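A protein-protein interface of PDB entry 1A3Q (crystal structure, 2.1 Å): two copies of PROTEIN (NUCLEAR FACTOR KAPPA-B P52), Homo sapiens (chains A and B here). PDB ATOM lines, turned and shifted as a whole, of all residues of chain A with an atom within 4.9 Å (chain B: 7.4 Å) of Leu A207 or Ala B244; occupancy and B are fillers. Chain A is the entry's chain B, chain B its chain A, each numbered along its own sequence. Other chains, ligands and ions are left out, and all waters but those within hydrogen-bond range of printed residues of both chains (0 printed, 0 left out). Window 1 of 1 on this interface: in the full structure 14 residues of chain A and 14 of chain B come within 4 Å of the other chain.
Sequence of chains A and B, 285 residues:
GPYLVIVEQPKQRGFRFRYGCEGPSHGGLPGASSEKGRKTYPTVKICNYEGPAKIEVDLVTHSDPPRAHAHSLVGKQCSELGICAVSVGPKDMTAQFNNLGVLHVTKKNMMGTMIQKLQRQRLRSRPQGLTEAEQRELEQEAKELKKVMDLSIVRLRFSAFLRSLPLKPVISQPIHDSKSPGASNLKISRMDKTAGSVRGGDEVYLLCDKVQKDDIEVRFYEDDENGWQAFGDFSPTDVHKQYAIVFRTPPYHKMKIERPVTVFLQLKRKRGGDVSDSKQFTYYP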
ATOM      1  N   LYS A 187      -6.194  -5.253  22.970  1.00  0.00           N
ATOM      2  CA  LYS A 187      -5.691  -6.413  22.217  1.00  0.00           C
ATOM      3  C   LYS A 187      -5.747  -6.260  20.681  1.00  0.00           C
ATOM      4  O   LYS A 187      -6.735  -5.771  20.105  1.00  0.00           O
ATOM      5  CB  LYS A 187      -6.441  -7.695  22.618  1.00  0.00           C
ATOM      6  CG  LYS A 187      -5.946  -8.968  21.891  1.00  0.00           C
ATOM      7  CD  LYS A 187      -6.893 -10.184  22.023  1.00  0.00           C
ATOM      8  CE  LYS A 187      -7.021 -10.679  23.479  1.00  0.00           C
ATOM      9  NZ  LYS A 187      -7.906 -11.885  23.616  1.00  0.00           N
ATOM     10  N   ILE A 188      -4.653  -6.650  20.034  1.00  0.00           N
ATOM     11  CA  ILE A 188      -4.543  -6.618  18.574  1.00  0.00           C
ATOM     12  C   ILE A 188      -4.865  -8.040  18.127  1.00  0.00           C
ATOM     13  O   ILE A 188      -4.091  -8.969  18.370  1.00  0.00           O
ATOM     14  CB  ILE A 188      -3.090  -6.225  18.066  1.00  0.00           C
ATOM     15  CG1 ILE A 188      -2.834  -4.723  18.272  1.00  0.00           C
ATOM     16  CG2 ILE A 188      -2.939  -6.577  16.584  1.00  0.00           C
ATOM     17  CD1 ILE A 188      -1.465  -4.248  17.918  1.00  0.00           C
ATOM     18  N   SER A 189      -6.036  -8.207  17.535  1.00  0.00           N
ATOM     19  CA  SER A 189      -6.472  -9.505  17.073  1.00  0.00           C
ATOM     20  C   SER A 189      -5.749  -9.977  15.812  1.00  0.00           C
ATOM     21  O   SER A 189      -4.994 -10.955  15.849  1.00  0.00           O
ATOM     22  CB  SER A 189      -7.978  -9.466  16.857  1.00  0.00           C
ATOM     23  OG  SER A 189      -8.445 -10.575  16.105  1.00  0.00           O
ATOM     24  N   ARG A 190      -6.038  -9.320  14.688  1.00  0.00           N
ATOM     25  CA  ARG A 190      -5.438  -9.641  13.387  1.00  0.00           C
ATOM     26  C   ARG A 190      -5.013  -8.364  12.697  1.00  0.00           C
ATOM     27  O   ARG A 190      -5.611  -7.303  12.904  1.00  0.00           O
ATOM     28  CB  ARG A 190      -6.447 -10.295  12.449  1.00  0.00           C
ATOM     29  CG  ARG A 190      -6.890 -11.644  12.833  1.00  0.00           C
ATOM     30  CD  ARG A 190      -7.844 -12.152  11.808  1.00  0.00           C
ATOM     31  NE  ARG A 190      -7.215 -13.176  11.002  1.00  0.00           N
ATOM     32  CZ  ARG A 190      -7.878 -14.183  10.447  1.00  0.00           C
ATOM     33  NH1 ARG A 190      -9.192 -14.283  10.623  1.00  0.00           N
ATOM     34  NH2 ARG A 190      -7.238 -15.065   9.686  1.00  0.00           N
ATOM     35  N   TYR A 205      -5.435  -2.556   7.903  1.00  0.00           N
ATOM     36  CA  TYR A 205      -6.722  -2.881   8.511  1.00  0.00           C
ATOM     37  C   TYR A 205      -6.393  -3.766   9.702  1.00  0.00           C
ATOM     38  O   TYR A 205      -6.080  -4.939   9.535  1.00  0.00           O
ATOM     39  CB  TYR A 205      -7.625  -3.679   7.563  1.00  0.00           C
ATOM     40  CG  TYR A 205      -8.436  -2.863   6.566  1.00  0.00           C
ATOM     41  CD1 TYR A 205      -7.896  -1.736   5.934  1.00  0.00           C
ATOM     42  CD2 TYR A 205      -9.752  -3.226   6.260  1.00  0.00           C
ATOM     43  CE1 TYR A 205      -8.631  -1.007   5.013  1.00  0.00           C
ATOM     44  CE2 TYR A 205     -10.492  -2.512   5.351  1.00  0.00           C
ATOM     45  CZ  TYR A 205      -9.929  -1.396   4.732  1.00  0.00           C
ATOM     46  OH  TYR A 205     -10.673  -0.702   3.804  1.00  0.00           O
ATOM     47  N   LEU A 206      -6.374  -3.165  10.887  1.00  0.00           N
ATOM     48  CA  LEU A 206      -6.119  -3.858  12.142  1.00  0.00           C
ATOM     49  C   LEU A 206      -7.467  -4.073  12.823  1.00  0.00           C
ATOM     50  O   LEU A 206      -8.331  -3.188  12.835  1.00  0.00           O
ATOM     51  CB  LEU A 206      -5.186  -3.021  13.030  1.00  0.00           C
ATOM     52  CG  LEU A 206      -5.156  -3.223  14.550  1.00  0.00           C
ATOM     53  CD1 LEU A 206      -4.842  -4.625  14.941  1.00  0.00           C
ATOM     54  CD2 LEU A 206      -4.119  -2.340  15.131  1.00  0.00           C
ATOM     55  N   LEU A 207      -7.680  -5.284  13.300  1.00  0.00           N
ATOM     56  CA  LEU A 207      -8.911  -5.619  13.983  1.00  0.00           C
ATOM     57  C   LEU A 207      -8.465  -5.783  15.414  1.00  0.00           C
ATOM     58  O   LEU A 207      -7.457  -6.447  15.687  1.00  0.00           O
ATOM     59  CB  LEU A 207      -9.502  -6.914  13.419  1.00  0.00           C
ATOM     60  CG  LEU A 207      -9.772  -6.908  11.919  1.00  0.00           C
ATOM     61  CD1 LEU A 207     -10.251  -8.241  11.492  1.00  0.00           C
ATOM     62  CD2 LEU A 207     -10.777  -5.871  11.592  1.00  0.00           C
ATOM     63  N   CYS A 208      -9.211  -5.186  16.331  1.00  0.00           N
ATOM     64  CA  CYS A 208      -8.832  -5.219  17.735  1.00  0.00           C
ATOM     65  C   CYS A 208     -10.031  -5.377  18.652  1.00  0.00           C
ATOM     66  O   CYS A 208     -11.169  -5.460  18.180  1.00  0.00           O
ATOM     67  CB  CYS A 208      -8.213  -3.871  18.050  1.00  0.00           C
ATOM     68  SG  CYS A 208      -9.278  -2.566  17.411  1.00  0.00           S
ATOM     69  N   ASP A 209      -9.754  -5.417  19.958  1.00  0.00           N
ATOM     70  CA  ASP A 209     -10.787  -5.469  20.999  1.00  0.00           C
ATOM     71  C   ASP A 209     -11.250  -4.008  21.199  1.00  0.00           C
ATOM     72  O   ASP A 209     -10.515  -3.075  20.885  1.00  0.00           O
ATOM     73  CB  ASP A 209     -10.231  -6.070  22.304  1.00  0.00           C
ATOM     74  CG  ASP A 209     -10.450  -7.594  22.401  1.00  0.00           C
ATOM     75  OD1 ASP A 209     -11.075  -8.233  21.508  1.00  0.00           O
ATOM     76  OD2 ASP A 209      -9.992  -8.176  23.404  1.00  0.00           O
ATOM     77  N   TYR A 243     -14.110  -1.610  16.957  1.00  0.00           N
ATOM     78  CA  TYR A 243     -13.419  -2.893  16.829  1.00  0.00           C
ATOM     79  C   TYR A 243     -12.480  -3.082  15.667  1.00  0.00           C
ATOM     80  O   TYR A 243     -12.056  -4.213  15.384  1.00  0.00           O
ATOM     81  CB  TYR A 243     -14.432  -4.018  16.774  1.00  0.00           C
ATOM     82  CG  TYR A 243     -15.177  -4.189  18.043  1.00  0.00           C
ATOM     83  CD1 TYR A 243     -14.538  -4.672  19.186  1.00  0.00           C
ATOM     84  CD2 TYR A 243     -16.527  -3.874  18.108  1.00  0.00           C
ATOM     85  CE1 TYR A 243     -15.233  -4.826  20.367  1.00  0.00           C
ATOM     86  CE2 TYR A 243     -17.231  -4.017  19.275  1.00  0.00           C
ATOM     87  CZ  TYR A 243     -16.591  -4.498  20.401  1.00  0.00           C
ATOM     88  OH  TYR A 243     -17.329  -4.657  21.550  1.00  0.00           O
ATOM     89  N   ALA A 244     -12.171  -1.997  14.982  1.00  0.00           N
ATOM     90  CA  ALA A 244     -11.268  -2.042  13.862  1.00  0.00           C
ATOM     91  C   ALA A 244     -10.693  -0.657  13.648  1.00  0.00           C
ATOM     92  O   ALA A 244     -11.354   0.351  13.880  1.00  0.00           O
ATOM     93  CB  ALA A 244     -12.017  -2.508  12.617  1.00  0.00           C
ATOM     94  N   TYR B 205     -10.385  -8.503   4.132  1.00  0.00           N
ATOM     95  CA  TYR B 205     -10.913  -8.011   5.400  1.00  0.00           C
ATOM     96  C   TYR B 205     -12.086  -7.097   4.999  1.00  0.00           C
ATOM     97  O   TYR B 205     -11.891  -6.085   4.327  1.00  0.00           O
ATOM     98  CB  TYR B 205      -9.890  -7.151   6.129  1.00  0.00           C
ATOM     99  CG  TYR B 205      -8.919  -7.894   7.014  1.00  0.00           C
ATOM    100  CD1 TYR B 205      -8.466  -9.165   6.682  1.00  0.00           C
ATOM    101  CD2 TYR B 205      -8.400  -7.303   8.151  1.00  0.00           C
ATOM    102  CE1 TYR B 205      -7.499  -9.804   7.442  1.00  0.00           C
ATOM    103  CE2 TYR B 205      -7.433  -7.944   8.925  1.00  0.00           C
ATOM    104  CZ  TYR B 205      -6.997  -9.199   8.567  1.00  0.00           C
ATOM    105  OH  TYR B 205      -6.059  -9.838   9.338  1.00  0.00           O
ATOM    106  N   LEU B 206     -13.300  -7.455   5.387  1.00  0.00           N
ATOM    107  CA  LEU B 206     -14.477  -6.678   5.062  1.00  0.00           C
ATOM    108  C   LEU B 206     -15.029  -6.058   6.335  1.00  0.00           C
ATOM    109  O   LEU B 206     -15.222  -6.764   7.318  1.00  0.00           O
ATOM    110  CB  LEU B 206     -15.504  -7.627   4.454  1.00  0.00           C
ATOM    111  CG  LEU B 206     -16.740  -7.068   3.764  1.00  0.00           C
ATOM    112  CD1 LEU B 206     -17.046  -7.893   2.558  1.00  0.00           C
ATOM    113  CD2 LEU B 206     -17.928  -7.115   4.706  1.00  0.00           C
ATOM    114  N   LEU B 207     -15.237  -4.742   6.343  1.00  0.00           N
ATOM    115  CA  LEU B 207     -15.801  -4.046   7.511  1.00  0.00           C
ATOM    116  C   LEU B 207     -17.284  -3.897   7.242  1.00  0.00           C
ATOM    117  O   LEU B 207     -17.669  -3.386   6.212  1.00  0.00           O
ATOM    118  CB  LEU B 207     -15.173  -2.655   7.704  1.00  0.00           C
ATOM    119  CG  LEU B 207     -13.652  -2.618   7.898  1.00  0.00           C
ATOM    120  CD1 LEU B 207     -13.274  -1.249   8.344  1.00  0.00           C
ATOM    121  CD2 LEU B 207     -13.175  -3.664   8.917  1.00  0.00           C
ATOM    122  N   CYS B 208     -18.129  -4.327   8.170  1.00  0.00           N
ATOM    123  CA  CYS B 208     -19.581  -4.253   7.961  1.00  0.00           C
ATOM    124  C   CYS B 208     -20.351  -3.757   9.181  1.00  0.00           C
ATOM    125  O   CYS B 208     -19.741  -3.464  10.210  1.00  0.00           O
ATOM    126  CB  CYS B 208     -20.107  -5.639   7.575  1.00  0.00           C
ATOM    127  SG  CYS B 208     -19.504  -6.964   8.625  1.00  0.00           S
ATOM    128  N   ASP B 209     -21.670  -3.562   9.031  1.00  0.00           N
ATOM    129  CA  ASP B 209     -22.512  -3.162  10.162  1.00  0.00           C
ATOM    130  C   ASP B 209     -22.724  -4.465  10.896  1.00  0.00           C
ATOM    131  O   ASP B 209     -22.471  -5.519  10.317  1.00  0.00           O
ATOM    132  CB  ASP B 209     -23.831  -2.582   9.680  1.00  0.00           C
ATOM    133  CG  ASP B 209     -23.762  -1.067   9.487  1.00  0.00           C
ATOM    134  OD1 ASP B 209     -22.888  -0.393  10.100  1.00  0.00           O
ATOM    135  OD2 ASP B 209     -24.575  -0.523   8.709  1.00  0.00           O
ATOM    136  N   LYS B 210     -23.168  -4.436  12.146  1.00  0.00           N
ATOM    137  CA  LYS B 210     -23.354  -5.678  12.912  1.00  0.00           C
ATOM    138  C   LYS B 210     -24.007  -6.873  12.207  1.00  0.00           C
ATOM    139  O   LYS B 210     -25.138  -6.778  11.713  1.00  0.00           O
ATOM    140  CB  LYS B 210     -24.126  -5.406  14.209  1.00  0.00           C
ATOM    141  CG  LYS B 210     -24.375  -6.686  15.060  1.00  0.00           C
ATOM    142  CD  LYS B 210     -24.992  -6.395  16.400  1.00  0.00           C
ATOM    143  CE  LYS B 210     -24.185  -5.367  17.150  1.00  0.00           C
ATOM    144  NZ  LYS B 210     -24.895  -4.950  18.362  1.00  0.00           N
ATOM    145  N   VAL B 211     -23.321  -8.009  12.179  1.00  0.00           N
ATOM    146  CA  VAL B 211     -23.905  -9.206  11.566  1.00  0.00           C
ATOM    147  C   VAL B 211     -23.748 -10.394  12.493  1.00  0.00           C
ATOM    148  O   VAL B 211     -22.876 -10.404  13.384  1.00  0.00           O
ATOM    149  CB  VAL B 211     -23.230  -9.598  10.235  1.00  0.00           C
ATOM    150  CG1 VAL B 211     -23.459  -8.521   9.192  1.00  0.00           C
ATOM    151  CG2 VAL B 211     -21.724  -9.882  10.461  1.00  0.00           C
ATOM    152  N   PRO B 236     -16.797 -18.969  11.774  1.00  0.00           N
ATOM    153  CA  PRO B 236     -17.291 -17.920  12.679  1.00  0.00           C
ATOM    154  C   PRO B 236     -16.182 -17.124  13.406  1.00  0.00           C
ATOM    155  O   PRO B 236     -16.378 -15.972  13.758  1.00  0.00           O
ATOM    156  CB  PRO B 236     -18.232 -18.694  13.628  1.00  0.00           C
ATOM    157  CG  PRO B 236     -17.854 -20.168  13.428  1.00  0.00           C
ATOM    158  CD  PRO B 236     -17.552 -20.222  11.973  1.00  0.00           C
ATOM    159  N   THR B 237     -15.008 -17.734  13.574  1.00  0.00           N
ATOM    160  CA  THR B 237     -13.867 -17.092  14.229  1.00  0.00           C
ATOM    161  C   THR B 237     -13.383 -15.952  13.356  1.00  0.00           C
ATOM    162  O   THR B 237     -12.705 -15.051  13.832  1.00  0.00           O
ATOM    163  CB  THR B 237     -12.667 -18.067  14.424  1.00  0.00           C
ATOM    164  OG1 THR B 237     -13.053 -19.406  14.100  1.00  0.00           O
ATOM    165  CG2 THR B 237     -12.206 -18.062  15.866  1.00  0.00           C
ATOM    166  N   ASP B 238     -13.693 -16.051  12.065  1.00  0.00           N
ATOM    167  CA  ASP B 238     -13.306 -15.051  11.080  1.00  0.00           C
ATOM    168  C   ASP B 238     -14.202 -13.846  11.088  1.00  0.00           C
ATOM    169  O   ASP B 238     -13.879 -12.853  10.454  1.00  0.00           O
ATOM    170  CB  ASP B 238     -13.261 -15.640   9.680  1.00  0.00           C
ATOM    171  CG  ASP B 238     -12.151 -16.623   9.524  1.00  0.00           C
ATOM    172  OD1 ASP B 238     -11.086 -16.400  10.117  1.00  0.00           O
ATOM    173  OD2 ASP B 238     -12.353 -17.649   8.856  1.00  0.00           O
ATOM    174  N   VAL B 239     -15.372 -13.977  11.713  1.00  0.00           N
ATOM    175  CA  VAL B 239     -16.302 -12.857  11.849  1.00  0.00           C
ATOM    176  C   VAL B 239     -15.883 -12.238  13.188  1.00  0.00           C
ATOM    177  O   VAL B 239     -16.098 -12.805  14.258  1.00  0.00           O
ATOM    178  CB  VAL B 239     -17.778 -13.300  11.888  1.00  0.00           C
ATOM    179  CG1 VAL B 239     -18.680 -12.081  11.951  1.00  0.00           C
ATOM    180  CG2 VAL B 239     -18.111 -14.152  10.668  1.00  0.00           C
ATOM    181  N   HIS B 240     -15.239 -11.081  13.107  1.00  0.00           N
ATOM    182  CA  HIS B 240     -14.711 -10.383  14.272  1.00  0.00           C
ATOM    183  C   HIS B 240     -15.661  -9.394  14.974  1.00  0.00           C
ATOM    184  O   HIS B 240     -16.020  -8.356  14.391  1.00  0.00           O
ATOM    185  CB  HIS B 240     -13.421  -9.677  13.833  1.00  0.00           C
ATOM    186  CG  HIS B 240     -12.838  -8.761  14.862  1.00  0.00           C
ATOM    187  ND1 HIS B 240     -12.010  -9.207  15.864  1.00  0.00           N
ATOM    188  CD2 HIS B 240     -12.852  -7.412  14.951  1.00  0.00           C
ATOM    189  CE1 HIS B 240     -11.514  -8.173  16.513  1.00  0.00           C
ATOM    190  NE2 HIS B 240     -12.009  -7.070  15.980  1.00  0.00           N
ATOM    191  N   LYS B 241     -16.056  -9.724  16.217  1.00  0.00           N
ATOM    192  CA  LYS B 241     -16.930  -8.874  17.046  1.00  0.00           C
ATOM    193  C   LYS B 241     -18.126  -8.294  16.268  1.00  0.00           C
ATOM    194  O   LYS B 241     -18.433  -7.108  16.405  1.00  0.00           O
ATOM    195  CB  LYS B 241     -16.100  -7.721  17.648  1.00  0.00           C
ATOM    196  CG  LYS B 241     -14.827  -8.161  18.424  1.00  0.00           C
ATOM    197  CD  LYS B 241     -15.173  -8.517  19.855  1.00  0.00           C
ATOM    198  CE  LYS B 241     -14.060  -9.194  20.593  1.00  0.00           C
ATOM    199  NZ  LYS B 241     -14.581  -9.586  21.936  1.00  0.00           N
ATOM    200  N   GLN B 242     -18.703  -9.109  15.376  1.00  0.00           N
ATOM    201  CA  GLN B 242     -19.860  -8.766  14.529  1.00  0.00           C
ATOM    202  C   GLN B 242     -19.725  -7.582  13.570  1.00  0.00           C
ATOM    203  O   GLN B 242     -20.702  -7.217  12.914  1.00  0.00           O
ATOM    204  CB  GLN B 242     -21.109  -8.568  15.398  1.00  0.00           C
ATOM    205  CG  GLN B 242     -21.475  -9.793  16.225  1.00  0.00           C
ATOM    206  CD  GLN B 242     -22.535  -9.516  17.273  1.00  0.00           C
ATOM    207  OE1 GLN B 242     -22.500  -8.510  17.985  1.00  0.00           O
ATOM    208  NE2 GLN B 242     -23.486 -10.422  17.376  1.00  0.00           N
ATOM    209  N   TYR B 243     -18.525  -7.020  13.455  1.00  0.00           N
ATOM    210  CA  TYR B 243     -18.268  -5.849  12.601  1.00  0.00           C
ATOM    211  C   TYR B 243     -17.195  -5.998  11.494  1.00  0.00           C
ATOM    212  O   TYR B 243     -16.839  -5.029  10.825  1.00  0.00           O
ATOM    213  CB  TYR B 243     -17.862  -4.677  13.492  1.00  0.00           C
ATOM    214  CG  TYR B 243     -18.968  -4.164  14.346  1.00  0.00           C
ATOM    215  CD1 TYR B 243     -20.088  -3.576  13.781  1.00  0.00           C
ATOM    216  CD2 TYR B 243     -18.896  -4.249  15.722  1.00  0.00           C
ATOM    217  CE1 TYR B 243     -21.119  -3.081  14.572  1.00  0.00           C
ATOM    218  CE2 TYR B 243     -19.920  -3.754  16.530  1.00  0.00           C
ATOM    219  CZ  TYR B 243     -21.022  -3.172  15.950  1.00  0.00           C
ATOM    220  OH  TYR B 243     -22.018  -2.660  16.745  1.00  0.00           O
ATOM    221  N   ALA B 244     -16.633  -7.188  11.361  1.00  0.00           N
ATOM    222  CA  ALA B 244     -15.615  -7.447  10.368  1.00  0.00           C
ATOM    223  C   ALA B 244     -15.672  -8.926  10.042  1.00  0.00           C
ATOM    224  O   ALA B 244     -16.049  -9.740  10.887  1.00  0.00           O
ATOM    225  CB  ALA B 244     -14.246  -7.093  10.904  1.00  0.00           C
ATOM    226  N   ILE B 245     -15.367  -9.238   8.785  1.00  0.00           N
ATOM    227  CA  ILE B 245     -15.312 -10.593   8.281  1.00  0.00           C
ATOM    228  C   ILE B 245     -13.990 -10.769   7.515  1.00  0.00           C
ATOM    229  O   ILE B 245     -13.673  -9.980   6.641  1.00  0.00           O
ATOM    230  CB  ILE B 245     -16.473 -10.884   7.311  1.00  0.00           C
ATOM    231  CG1 ILE B 245     -17.802 -10.545   7.975  1.00  0.00           C
ATOM    232  CG2 ILE B 245     -16.464 -12.363   6.913  1.00  0.00           C
ATOM    233  CD1 ILE B 245     -18.972 -10.773   7.053  1.00  0.00           C
ATOM    234  N   VAL B 246     -13.188 -11.748   7.904  1.00  0.00           N
ATOM    235  CA  VAL B 246     -11.940 -12.026   7.206  1.00  0.00           C
ATOM    236  C   VAL B 246     -12.250 -13.288   6.431  1.00  0.00           C
ATOM    237  O   VAL B 246     -12.504 -14.333   7.009  1.00  0.00           O
ATOM    238  CB  VAL B 246     -10.731 -12.265   8.183  1.00  0.00           C
ATOM    239  CG1 VAL B 246      -9.486 -12.682   7.422  1.00  0.00           C
ATOM    240  CG2 VAL B 246     -10.414 -10.997   8.979  1.00  0.00           C
ATOM    241  N   PHE B 247     -12.301 -13.161   5.111  1.00  0.00           N
ATOM    242  CA  PHE B 247     -12.604 -14.294   4.262  1.00  0.00           C
ATOM    243  C   PHE B 247     -11.639 -14.464   3.092  1.00  0.00           C
ATOM    244  O   PHE B 247     -10.972 -13.512   2.668  1.00  0.00           O
ATOM    245  CB  PHE B 247     -14.030 -14.158   3.719  1.00  0.00           C
ATOM    246  CG  PHE B 247     -14.207 -13.059   2.700  1.00  0.00           C
ATOM    247  CD1 PHE B 247     -14.445 -11.759   3.090  1.00  0.00           C
ATOM    248  CD2 PHE B 247     -14.196 -13.353   1.334  1.00  0.00           C
ATOM    249  CE1 PHE B 247     -14.673 -10.760   2.140  1.00  0.00           C
ATOM    250  CE2 PHE B 247     -14.421 -12.372   0.387  1.00  0.00           C
ATOM    251  CZ  PHE B 247     -14.664 -11.069   0.790  1.00  0.00           C
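Of the printed residues of chain B, Leu A207 touches Tyr B205 (3.8 Å), His B240 (3.6 Å), Ala B244 (3.7 Å) and Val B246 (3.7 Å). Of the printed residues of chain B, Asp A209 touches Lys B241 (3.3 Å). Val B239 touches none of the printed residues of chain A. Of chain A, only Leu A207 comes within 4 Å of Ala B244. Of the printed residues of chain A, Val B246 touches Arg A190 and Leu A207. The nearest printed residue of chain A that does not touch Ala B244 is Ala A244 (5.4 Å).
Tyr A205 touches its own counterpart, Tyr B205. Leu A207 touches Tyr B205, but with the chains exchanged Tyr A205 does not touch Leu B207 (4.1 Å). Leu A207 touches Ala B244, but with the chains exchanged Ala A244 does not touch Leu B207 (4.05 Å). Tyr A243 touches its own counterpart, Tyr B243. 7 positions are printed for both chains. Of the 14 pairs that touch across the chains among the printed residues, 2 have their exchanged pair printed and touching as well.
Printed residues of chain B that touch a printed residue of chain A: Tyr B205, Asp B238, His B240, Lys B241, Tyr B243, Ala B244 and Val B246. Hydrophobic or aromatic side chains of chain B that line the printed part of chain A: Tyr B205, His B240, Tyr B243, Ala B244 and Val B246. Of the 11 printed residues of chain A, 7 touch a printed residue of chain B. Hydrophobic or aromatic side chains of chain A within 4 Å of the printed part of chain B: Tyr A205, Leu A207 and Tyr A243.
O of Tyr B243 sits at hydrogen-bond distance from N of Cys B208 (3.0 Å). The backbone carbonyl oxygen of Asp B238 lies within hydrogen-bond range of the backbone NH of Val B246, at 2.9 Å. N of Asp A209 lies within hydrogen-bond range of O of Lys A187. The backbone NH (N) of Ser A189 lies within hydrogen-bond range of the backbone carbonyl oxygen (O) of Leu A207, at 2.9 Å. The backbone NH (N) of Leu A207 lies within hydrogen-bond range of the backbone carbonyl oxygen (O) of Arg A190 (2.9 Å). The backbone NH (N) of Cys A208 lies within hydrogen-bond range of the backbone carbonyl oxygen (O) of Tyr A243 (3.2 Å).
His B240 touches Ser A189 (CE1 to CB, 3.8 Å). Tyr B205 touches Arg A190 (OH to CB, 3.2 Å). Arg A190 touches Val B246. Tyr A205 touches Tyr B205 (O to CE2, 3.4 Å). CE2 of Tyr B205 touches CD1 of Leu A207 (3.8 Å). Leu A207 touches His B240. CB of Ala B244 touches CD2 of Leu A207, at 3.7 Å. CD1 of Leu A207 touches CG2 of Val B246, 3.7 Å away. Tyr A243 touches Lys B241. Tyr A243 touches Tyr B243.
NH1 of Arg A190 is in salt-bridge range of OD1 of Asp B238 (2.9 Å). A ring nitrogen (NE2) of His B240 sits at hydrogen-bond distance from the backbone carbonyl oxygen of Cys A208, at 2.9 Å. A ring nitrogen (NE2) of His B240 lies within hydrogen-bond range of the backbone carbonyl oxygen (O) of Tyr A243, 2.9 Å away. The side-chain carboxylate of Asp A209 lies within salt-bridge range of the side-chain amino group of Lys B241, at 3.8 Å.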
